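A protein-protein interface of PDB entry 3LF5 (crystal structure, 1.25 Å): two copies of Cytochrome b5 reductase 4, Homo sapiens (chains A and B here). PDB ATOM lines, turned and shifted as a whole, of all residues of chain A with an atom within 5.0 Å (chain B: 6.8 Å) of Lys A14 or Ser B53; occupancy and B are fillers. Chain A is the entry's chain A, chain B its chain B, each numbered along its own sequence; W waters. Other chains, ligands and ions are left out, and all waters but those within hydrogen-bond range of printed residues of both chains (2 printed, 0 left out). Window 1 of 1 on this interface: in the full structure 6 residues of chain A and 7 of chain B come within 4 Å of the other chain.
OE2 of Glu A10 is in salt-bridge range of NH2 of Arg B49 (2.9 Å).
O of Arg B49 lies within hydrogen-bond range of NZ of Lys A14, 3.2 Å away.
The side-chain amino group (NZ) of Lys A14 lies within hydrogen-bond range of the backbone carbonyl oxygen (O) of Ala B51 (2.9 Å).
O of Asn A17 sits at hydrogen-bond distance from NZ of Lys B14.
N of Cys B25 is in hydrogen-bond range of O of Ser B53 (3.0 Å).
OG of Ser B53 lies within hydrogen-bond range of O of Ala B50 (2.7 Å).
Among the printed residues, pairs that only touch across the chains: Lys A14 with Ser B53 (3.7 Å), Lys A14 with Met B48 (3.8 Å) and Lys A14 with Ala B50 (3.9 Å).
Of the printed residues of chain B, Lys A14 touches Met B48 (3.8 Å), Arg B49 (3.2 Å), Ala B50 (3.9 Å), Ala B51 (2.9 Å) and Ser B53 (3.7 Å).
His A16 touches none of the printed residues of chain B.
Of the printed residues of chain B, Asn A17 touches Lys B14 (2.8 Å).
Of the printed residues of chain A, Lys B14 touches Asn A17.
Of the printed residues of chain A, Arg B49 touches Glu A10 (2.9 Å) and Lys A14 (3.2 Å).
Of the printed residues of chain A, Ala B50 touches Lys A14 (3.9 Å).
Of the printed residues of chain A, Ala B51 touches Lys A14.
Of the 18 printed residues of chain B, 6 touch a printed residue of chain A.
Among the printed residues, Asp or Glu carboxylates within 4 Å of a Lys or Arg side-chain nitrogen of the other chain: Glu A10 with Arg B49 (2.9 Å).
Asn A17 touches Lys B14, but with the chains exchanged Lys A14 does not touch Asn B17 (6.1 Å).
Positions printed for both chains: 13, 14, 16, 17 and 52.
Of the 7 pairs that touch across the chains among the printed residues, none has its exchanged pair printed and touching as well.
Water W2 lies within hydrogen-bond range of the backbone carbonyl oxygen (O) of Gly B52 (3.0 Å), the backbone carbonyl oxygen (O) of Lys B14 (3.0 Å) and the side-chain amide nitrogen (ND2) of Asn A17 (3.1 Å).
Water W1 bridges O of Gly B52 (3.0 Å) and ND2 of Asn A17 (3.0 Å).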
ATOM      1  N   GLU A  10       7.012 -19.297  12.203  1.00  0.00           N
ATOM      2  CA  GLU A  10       5.806 -18.571  11.800  1.00  0.00           C
ATOM      3  C   GLU A  10       6.120 -17.101  11.525  1.00  0.00           C
ATOM      4  O   GLU A  10       5.568 -16.507  10.611  1.00  0.00           O
ATOM      5  CB  GLU A  10       4.684 -18.695  12.824  1.00  0.00           C
ATOM      6  CG  GLU A  10       3.925 -19.983  12.679  1.00  0.00           C
ATOM      7  CD  GLU A  10       2.683 -20.043  13.522  1.00  0.00           C
ATOM      8  OE1 GLU A  10       2.095 -18.976  13.824  1.00  0.00           O
ATOM      9  OE2 GLU A  10       2.270 -21.170  13.889  1.00  0.00           O
ATOM     10  N   GLU A  11       7.029 -16.513  12.297  1.00  0.00           N
ATOM     11  CA  GLU A  11       7.435 -15.127  12.051  1.00  0.00           C
ATOM     12  C   GLU A  11       8.028 -14.965  10.642  1.00  0.00           C
ATOM     13  O   GLU A  11       7.722 -14.004   9.932  1.00  0.00           O
ATOM     14  CB  GLU A  11       8.475 -14.714  13.089  1.00  0.00           C
ATOM     15  CG  GLU A  11       8.912 -13.269  13.021  1.00  0.00           C
ATOM     16  CD  GLU A  11       9.893 -12.914  14.135  1.00  0.00           C
ATOM     17  OE1 GLU A  11      10.454 -11.799  14.082  1.00  0.00           O
ATOM     18  OE2 GLU A  11      10.104 -13.754  15.054  1.00  0.00           O
ATOM     19  N   GLU A  12       8.852 -15.923  10.212  1.00  0.00           N
ATOM     20  CA  GLU A  12       9.398 -15.879   8.860  1.00  0.00           C
ATOM     21  C   GLU A  12       8.301 -16.076   7.818  1.00  0.00           C
ATOM     22  O   GLU A  12       8.211 -15.331   6.853  1.00  0.00           O
ATOM     23  CB  GLU A  12      10.495 -16.920   8.680  1.00  0.00           C
ATOM     24  CG  GLU A  12      11.128 -16.951   7.291  1.00  0.00           C
ATOM     25  CD  GLU A  12      11.903 -15.679   6.943  1.00  0.00           C
ATOM     26  OE1 GLU A  12      12.491 -15.034   7.849  1.00  0.00           O
ATOM     27  OE2 GLU A  12      11.953 -15.346   5.730  1.00  0.00           O
ATOM     28  N   LEU A  13       7.460 -17.081   8.024  1.00  0.00           N
ATOM     29  CA  LEU A  13       6.393 -17.387   7.066  1.00  0.00           C
ATOM     30  C   LEU A  13       5.544 -16.168   6.753  1.00  0.00           C
ATOM     31  O   LEU A  13       5.227 -15.888   5.598  1.00  0.00           O
ATOM     32  CB  LEU A  13       5.505 -18.520   7.619  1.00  0.00           C
ATOM     33  CG  LEU A  13       4.335 -18.971   6.726  1.00  0.00           C
ATOM     34  CD1 LEU A  13       4.835 -19.609   5.428  1.00  0.00           C
ATOM     35  CD2 LEU A  13       3.442 -19.955   7.519  1.00  0.00           C
ATOM     36  N   LYS A  14       5.184 -15.439   7.808  1.00  0.00           N
ATOM     37  CA  LYS A  14       4.262 -14.320   7.624  1.00  0.00           C
ATOM     38  C   LYS A  14       4.848 -13.147   6.850  1.00  0.00           C
ATOM     39  O   LYS A  14       4.093 -12.320   6.346  1.00  0.00           O
ATOM     40  CB  LYS A  14       3.747 -13.820   8.956  1.00  0.00           C
ATOM     41  CG  LYS A  14       2.910 -14.794   9.668  1.00  0.00           C
ATOM     42  CD  LYS A  14       2.654 -14.337  11.095  1.00  0.00           C
ATOM     43  CE  LYS A  14       2.007 -12.965  11.161  1.00  0.00           C
ATOM     44  NZ  LYS A  14       0.632 -13.038  10.604  1.00  0.00           N
ATOM     45  N   LYS A  15       6.174 -13.088   6.701  1.00  0.00           N
ATOM     46  CA  LYS A  15       6.797 -12.055   5.868  1.00  0.00           C
ATOM     47  C   LYS A  15       6.475 -12.252   4.382  1.00  0.00           C
ATOM     48  O   LYS A  15       6.539 -11.323   3.576  1.00  0.00           O
ATOM     49  CB  LYS A  15       8.316 -12.100   6.015  1.00  0.00           C
ATOM     50  CG  LYS A  15       8.831 -11.772   7.388  1.00  0.00           C
ATOM     51  CD  LYS A  15      10.339 -11.991   7.459  1.00  0.00           C
ATOM     52  CE  LYS A  15      10.894 -11.607   8.822  1.00  0.00           C
ATOM     53  NZ  LYS A  15      10.469 -12.524   9.915  1.00  0.00           N
ATOM     54  N   HIS A  16       6.171 -13.483   4.007  1.00  0.00           N
ATOM     55  CA  HIS A  16       5.978 -13.843   2.610  1.00  0.00           C
ATOM     56  C   HIS A  16       4.488 -13.914   2.310  1.00  0.00           C
ATOM     57  O   HIS A  16       3.920 -14.987   2.053  1.00  0.00           O
ATOM     58  CB  HIS A  16       6.704 -15.156   2.327  1.00  0.00           C
ATOM     59  CG  HIS A  16       8.143 -15.104   2.690  1.00  0.00           C
ATOM     60  ND1 HIS A  16       9.132 -14.746   1.796  1.00  0.00           N
ATOM     61  CD2 HIS A  16       8.762 -15.343   3.863  1.00  0.00           C
ATOM     62  CE1 HIS A  16      10.299 -14.767   2.416  1.00  0.00           C
ATOM     63  NE2 HIS A  16      10.100 -15.142   3.668  1.00  0.00           N
ATOM     64  N   ASN A  17       3.850 -12.747   2.367  1.00  0.00           N
ATOM     65  CA  ASN A  17       2.387 -12.660   2.307  1.00  0.00           C
ATOM     66  C   ASN A  17       1.926 -11.775   1.154  1.00  0.00           C
ATOM     67  O   ASN A  17       0.822 -11.236   1.204  1.00  0.00           O
ATOM     68  CB  ASN A  17       1.800 -12.192   3.649  1.00  0.00           C
ATOM     69  CG  ASN A  17       2.191 -10.761   3.979  1.00  0.00           C
ATOM     70  OD1 ASN A  17       3.098 -10.215   3.370  1.00  0.00           O
ATOM     71  ND2 ASN A  17       1.508 -10.160   4.937  1.00  0.00           N
ATOM     72  N   GLY A  52       1.298 -16.308   3.327  1.00  0.00           N
ATOM     73  CA  GLY A  52       2.015 -16.114   4.557  1.00  0.00           C
ATOM     74  C   GLY A  52       1.423 -16.857   5.727  1.00  0.00           C
ATOM     75  O   GLY A  52       1.590 -16.428   6.867  1.00  0.00           O
ATOM     76  N   LEU B  13      -4.752  -4.133   5.871  1.00  0.00           N
ATOM     77  CA  LEU B  13      -4.639  -5.018   7.030  1.00  0.00           C
ATOM     78  C   LEU B  13      -3.175  -5.449   7.209  1.00  0.00           C
ATOM     79  O   LEU B  13      -2.662  -5.461   8.326  1.00  0.00           O
ATOM     80  CB  LEU B  13      -5.499  -6.263   6.824  1.00  0.00           C
ATOM     81  CG  LEU B  13      -5.455  -7.338   7.900  1.00  0.00           C
ATOM     82  CD1 LEU B  13      -5.879  -6.839   9.249  1.00  0.00           C
ATOM     83  CD2 LEU B  13      -6.258  -8.544   7.470  1.00  0.00           C
ATOM     84  N   LYS B  14      -2.513  -5.808   6.114  1.00  0.00           N
ATOM     85  CA  LYS B  14      -1.168  -6.355   6.185  1.00  0.00           C
ATOM     86  C   LYS B  14      -0.141  -5.375   6.673  1.00  0.00           C
ATOM     87  O   LYS B  14       0.894  -5.773   7.177  1.00  0.00           O
ATOM     88  CB  LYS B  14      -0.756  -6.913   4.821  1.00  0.00           C
ATOM     89  CG  LYS B  14      -1.523  -8.159   4.467  1.00  0.00           C
ATOM     90  CD  LYS B  14      -1.223  -8.635   3.061  1.00  0.00           C
ATOM     91  CE  LYS B  14      -2.063  -9.863   2.720  1.00  0.00           C
ATOM     92  NZ  LYS B  14      -1.814 -10.323   1.310  1.00  0.00           N
ATOM     93  N   HIS B  16      -0.492  -3.472   9.244  1.00  0.00           N
ATOM     94  CA  HIS B  16      -0.568  -3.308  10.693  1.00  0.00           C
ATOM     95  C   HIS B  16      -0.145  -4.618  11.316  1.00  0.00           C
ATOM     96  O   HIS B  16      -0.948  -5.363  11.860  1.00  0.00           O
ATOM     97  CB  HIS B  16      -1.967  -2.922  11.085  1.00  0.00           C
ATOM     98  CG  HIS B  16      -2.394  -1.637  10.482  1.00  0.00           C
ATOM     99  ND1 HIS B  16      -2.263  -0.431  11.137  1.00  0.00           N
ATOM    100  CD2 HIS B  16      -2.922  -1.358   9.267  1.00  0.00           C
ATOM    101  CE1 HIS B  16      -2.683   0.536  10.336  1.00  0.00           C
ATOM    102  NE2 HIS B  16      -3.091  -0.001   9.201  1.00  0.00           N
ATOM    103  N   ASN B  17       1.163  -4.877  11.230  1.00  0.00           N
ATOM    104  CA  ASN B  17       1.746  -6.160  11.609  1.00  0.00           C
ATOM    105  C   ASN B  17       2.784  -6.064  12.711  1.00  0.00           C
ATOM    106  O   ASN B  17       3.527  -7.000  12.937  1.00  0.00           O
ATOM    107  CB  ASN B  17       2.321  -6.864  10.367  1.00  0.00           C
ATOM    108  CG  ASN B  17       3.502  -6.157   9.787  1.00  0.00           C
ATOM    109  OD1 ASN B  17       3.753  -5.018  10.085  1.00  0.00           O
ATOM    110  ND2 ASN B  17       4.256  -6.849   8.946  1.00  0.00           N
ATOM    111  N   TRP B  23      -3.185  -5.144  13.783  1.00  0.00           N
ATOM    112  CA  TRP B  23      -4.584  -5.392  13.431  1.00  0.00           C
ATOM    113  C   TRP B  23      -4.739  -6.880  13.141  1.00  0.00           C
ATOM    114  O   TRP B  23      -3.894  -7.493  12.508  1.00  0.00           O
ATOM    115  CB  TRP B  23      -5.068  -4.599  12.207  1.00  0.00           C
ATOM    116  CG  TRP B  23      -5.163  -3.118  12.341  1.00  0.00           C
ATOM    117  CD1 TRP B  23      -4.735  -2.341  13.360  1.00  0.00           C
ATOM    118  CD2 TRP B  23      -5.692  -2.231  11.343  1.00  0.00           C
ATOM    119  NE1 TRP B  23      -4.987  -1.012  13.079  1.00  0.00           N
ATOM    120  CE2 TRP B  23      -5.562  -0.921  11.838  1.00  0.00           C
ATOM    121  CE3 TRP B  23      -6.241  -2.423  10.076  1.00  0.00           C
ATOM    122  CZ2 TRP B  23      -5.967   0.183  11.115  1.00  0.00           C
ATOM    123  CZ3 TRP B  23      -6.644  -1.312   9.366  1.00  0.00           C
ATOM    124  CH2 TRP B  23      -6.503  -0.039   9.886  1.00  0.00           C
ATOM    125  N   ILE B  24      -5.853  -7.435  13.602  1.00  0.00           N
ATOM    126  CA  ILE B  24      -6.219  -8.829  13.353  1.00  0.00           C
ATOM    127  C   ILE B  24      -7.667  -8.848  12.887  1.00  0.00           C
ATOM    128  O   ILE B  24      -8.518  -8.178  13.465  1.00  0.00           O
ATOM    129  CB  ILE B  24      -6.060  -9.741  14.616  1.00  0.00           C
ATOM    130  CG1 ILE B  24      -4.635  -9.697  15.149  1.00  0.00           C
ATOM    131  CG2 ILE B  24      -6.546 -11.178  14.308  1.00  0.00           C
ATOM    132  CD1 ILE B  24      -4.426 -10.505  16.437  1.00  0.00           C
ATOM    133  N   CYS B  25      -7.937  -9.636  11.848  1.00  0.00           N
ATOM    134  CA  CYS B  25      -9.308  -9.863  11.417  1.00  0.00           C
ATOM    135  C   CYS B  25      -9.823 -11.166  11.991  1.00  0.00           C
ATOM    136  O   CYS B  25      -9.176 -12.197  11.890  1.00  0.00           O
ATOM    137  CB  CYS B  25      -9.347  -9.908   9.904  1.00  0.00           C
ATOM    138  SG  CYS B  25     -10.893 -10.404   9.184  1.00  0.00           S
ATOM    139  N   ILE B  26     -10.981 -11.120  12.631  1.00  0.00           N
ATOM    140  CA  ILE B  26     -11.666 -12.335  13.115  1.00  0.00           C
ATOM    141  C   ILE B  26     -13.081 -12.316  12.549  1.00  0.00           C
ATOM    142  O   ILE B  26     -13.875 -11.403  12.831  1.00  0.00           O
ATOM    143  CB  ILE B  26     -11.710 -12.390  14.658  1.00  0.00           C
ATOM    144  CG1 ILE B  26     -10.322 -12.264  15.284  1.00  0.00           C
ATOM    145  CG2 ILE B  26     -12.463 -13.649  15.125  1.00  0.00           C
ATOM    146  CD1 ILE B  26      -9.483 -13.476  15.279  1.00  0.00           C
ATOM    147  N   MET B  48       0.600 -12.240  18.383  1.00  0.00           N
ATOM    148  CA  MET B  48       1.395 -11.821  17.213  1.00  0.00           C
ATOM    149  C   MET B  48       1.410 -12.819  16.069  1.00  0.00           C
ATOM    150  O   MET B  48       1.731 -12.463  14.934  1.00  0.00           O
ATOM    151  CB  MET B  48       2.830 -11.483  17.618  1.00  0.00           C
ATOM    152  CG  MET B  48       2.981 -10.153  18.321  1.00  0.00           C
ATOM    153  SD  MET B  48       2.512  -8.743  17.286  1.00  0.00           S
ATOM    154  CE  MET B  48       3.852  -8.763  16.076  1.00  0.00           C
ATOM    155  N   ARG B  49       1.073 -14.073  16.350  1.00  0.00           N
ATOM    156  CA  ARG B  49       0.939 -15.063  15.302  1.00  0.00           C
ATOM    157  C   ARG B  49      -0.066 -14.653  14.235  1.00  0.00           C
ATOM    158  O   ARG B  49       0.018 -15.055  13.068  1.00  0.00           O
ATOM    159  CB  ARG B  49       0.559 -16.424  15.872  1.00  0.00           C
ATOM    160  CG  ARG B  49       1.599 -17.018  16.807  1.00  0.00           C
ATOM    161  CD  ARG B  49       1.104 -18.261  17.525  1.00  0.00           C
ATOM    162  NE  ARG B  49       0.908 -19.319  16.548  1.00  0.00           N
ATOM    163  CZ  ARG B  49       0.171 -20.410  16.726  1.00  0.00           C
ATOM    164  NH1 ARG B  49      -0.472 -20.611  17.864  1.00  0.00           N
ATOM    165  NH2 ARG B  49       0.063 -21.271  15.731  1.00  0.00           N
ATOM    166  N   ALA B  50      -1.036 -13.841  14.633  1.00  0.00           N
ATOM    167  CA  ALA B  50      -2.114 -13.395  13.729  1.00  0.00           C
ATOM    168  C   ALA B  50      -1.941 -11.947  13.270  1.00  0.00           C
ATOM    169  O   ALA B  50      -2.800 -11.400  12.591  1.00  0.00           O
ATOM    170  CB  ALA B  50      -3.480 -13.553  14.402  1.00  0.00           C
ATOM    171  N   ALA B  51      -0.821 -11.327  13.614  1.00  0.00           N
ATOM    172  CA  ALA B  51      -0.614  -9.903  13.322  1.00  0.00           C
ATOM    173  C   ALA B  51      -0.775  -9.617  11.839  1.00  0.00           C
ATOM    174  O   ALA B  51      -0.197 -10.310  11.000  1.00  0.00           O
ATOM    175  CB  ALA B  51       0.753  -9.437  13.807  1.00  0.00           C
ATOM    176  N   GLY B  52      -1.525  -8.567  11.516  1.00  0.00           N
ATOM    177  CA  GLY B  52      -1.665  -8.145  10.152  1.00  0.00           C
ATOM    178  C   GLY B  52      -2.263  -9.201   9.245  1.00  0.00           C
ATOM    179  O   GLY B  52      -1.915  -9.283   8.083  1.00  0.00           O
ATOM    180  N   SER B  53      -3.194  -9.987   9.763  1.00  0.00           N
ATOM    181  CA  SER B  53      -3.736 -11.114   9.038  1.00  0.00           C
ATOM    182  C   SER B  53      -5.114 -11.485   9.532  1.00  0.00           C
ATOM    183  O   SER B  53      -5.631 -10.970  10.524  1.00  0.00           O
ATOM    184  CB  SER B  53      -2.820 -12.320   9.169  1.00  0.00           C
ATOM    185  OG  SER B  53      -3.064 -12.977  10.386  1.00  0.00           O
ATOM    186  N   ASP B  54      -5.700 -12.429   8.829  1.00  0.00           N
ATOM    187  CA  ASP B  54      -6.928 -13.050   9.266  1.00  0.00           C
ATOM    188  C   ASP B  54      -6.587 -14.109  10.305  1.00  0.00           C
ATOM    189  O   ASP B  54      -5.988 -15.134   9.971  1.00  0.00           O
ATOM    190  CB  ASP B  54      -7.638 -13.705   8.074  1.00  0.00           C
ATOM    191  CG  ASP B  54      -9.050 -14.089   8.423  1.00  0.00           C
ATOM    192  OD1 ASP B  54      -9.283 -14.738   9.450  1.00  0.00           O
ATOM    193  OD2 ASP B  54      -9.970 -13.689   7.698  1.00  0.00           O
ATOM    194  N   GLY B  55      -6.973 -13.846  11.539  1.00  0.00           N
ATOM    195  CA  GLY B  55      -6.697 -14.732  12.622  1.00  0.00           C
ATOM    196  C   GLY B  55      -7.802 -15.704  12.987  1.00  0.00           C
ATOM    197  O   GLY B  55      -7.703 -16.369  14.008  1.00  0.00           O
ATOM    198  N   THR B  56      -8.845 -15.808  12.173  1.00  0.00           N
ATOM    199  CA  THR B  56     -10.001 -16.631  12.525  1.00  0.00           C
ATOM    200  C   THR B  56      -9.649 -18.087  12.783  1.00  0.00           C
ATOM    201  O   THR B  56     -10.074 -18.688  13.760  1.00  0.00           O
ATOM    202  CB  THR B  56     -11.068 -16.573  11.421  1.00  0.00           C
ATOM    203  OG1 THR B  56     -11.362 -15.207  11.091  1.00  0.00           O
ATOM    204  CG2 THR B  56     -12.329 -17.274  11.885  1.00  0.00           C
ATOM    205  N   LEU B  58      -6.701 -19.454  13.584  1.00  0.00           N
ATOM    206  CA  LEU B  58      -5.904 -19.590  14.792  1.00  0.00           C
ATOM    207  C   LEU B  58      -6.774 -19.438  16.036  1.00  0.00           C
ATOM    208  O   LEU B  58      -6.654 -20.198  16.992  1.00  0.00           O
ATOM    209  CB  LEU B  58      -4.817 -18.520  14.785  1.00  0.00           C
ATOM    210  CG  LEU B  58      -3.627 -18.759  13.859  1.00  0.00           C
ATOM    211  CD1 LEU B  58      -2.803 -17.486  13.702  1.00  0.00           C
ATOM    212  CD2 LEU B  58      -2.767 -19.911  14.343  1.00  0.00           C
HETATM  213  O   HOH W   1      -0.930 -11.413   6.205  1.00  0.00           O
HETATM  214  O   HOH W   2       0.985  -8.745   7.620  1.00  0.00           O
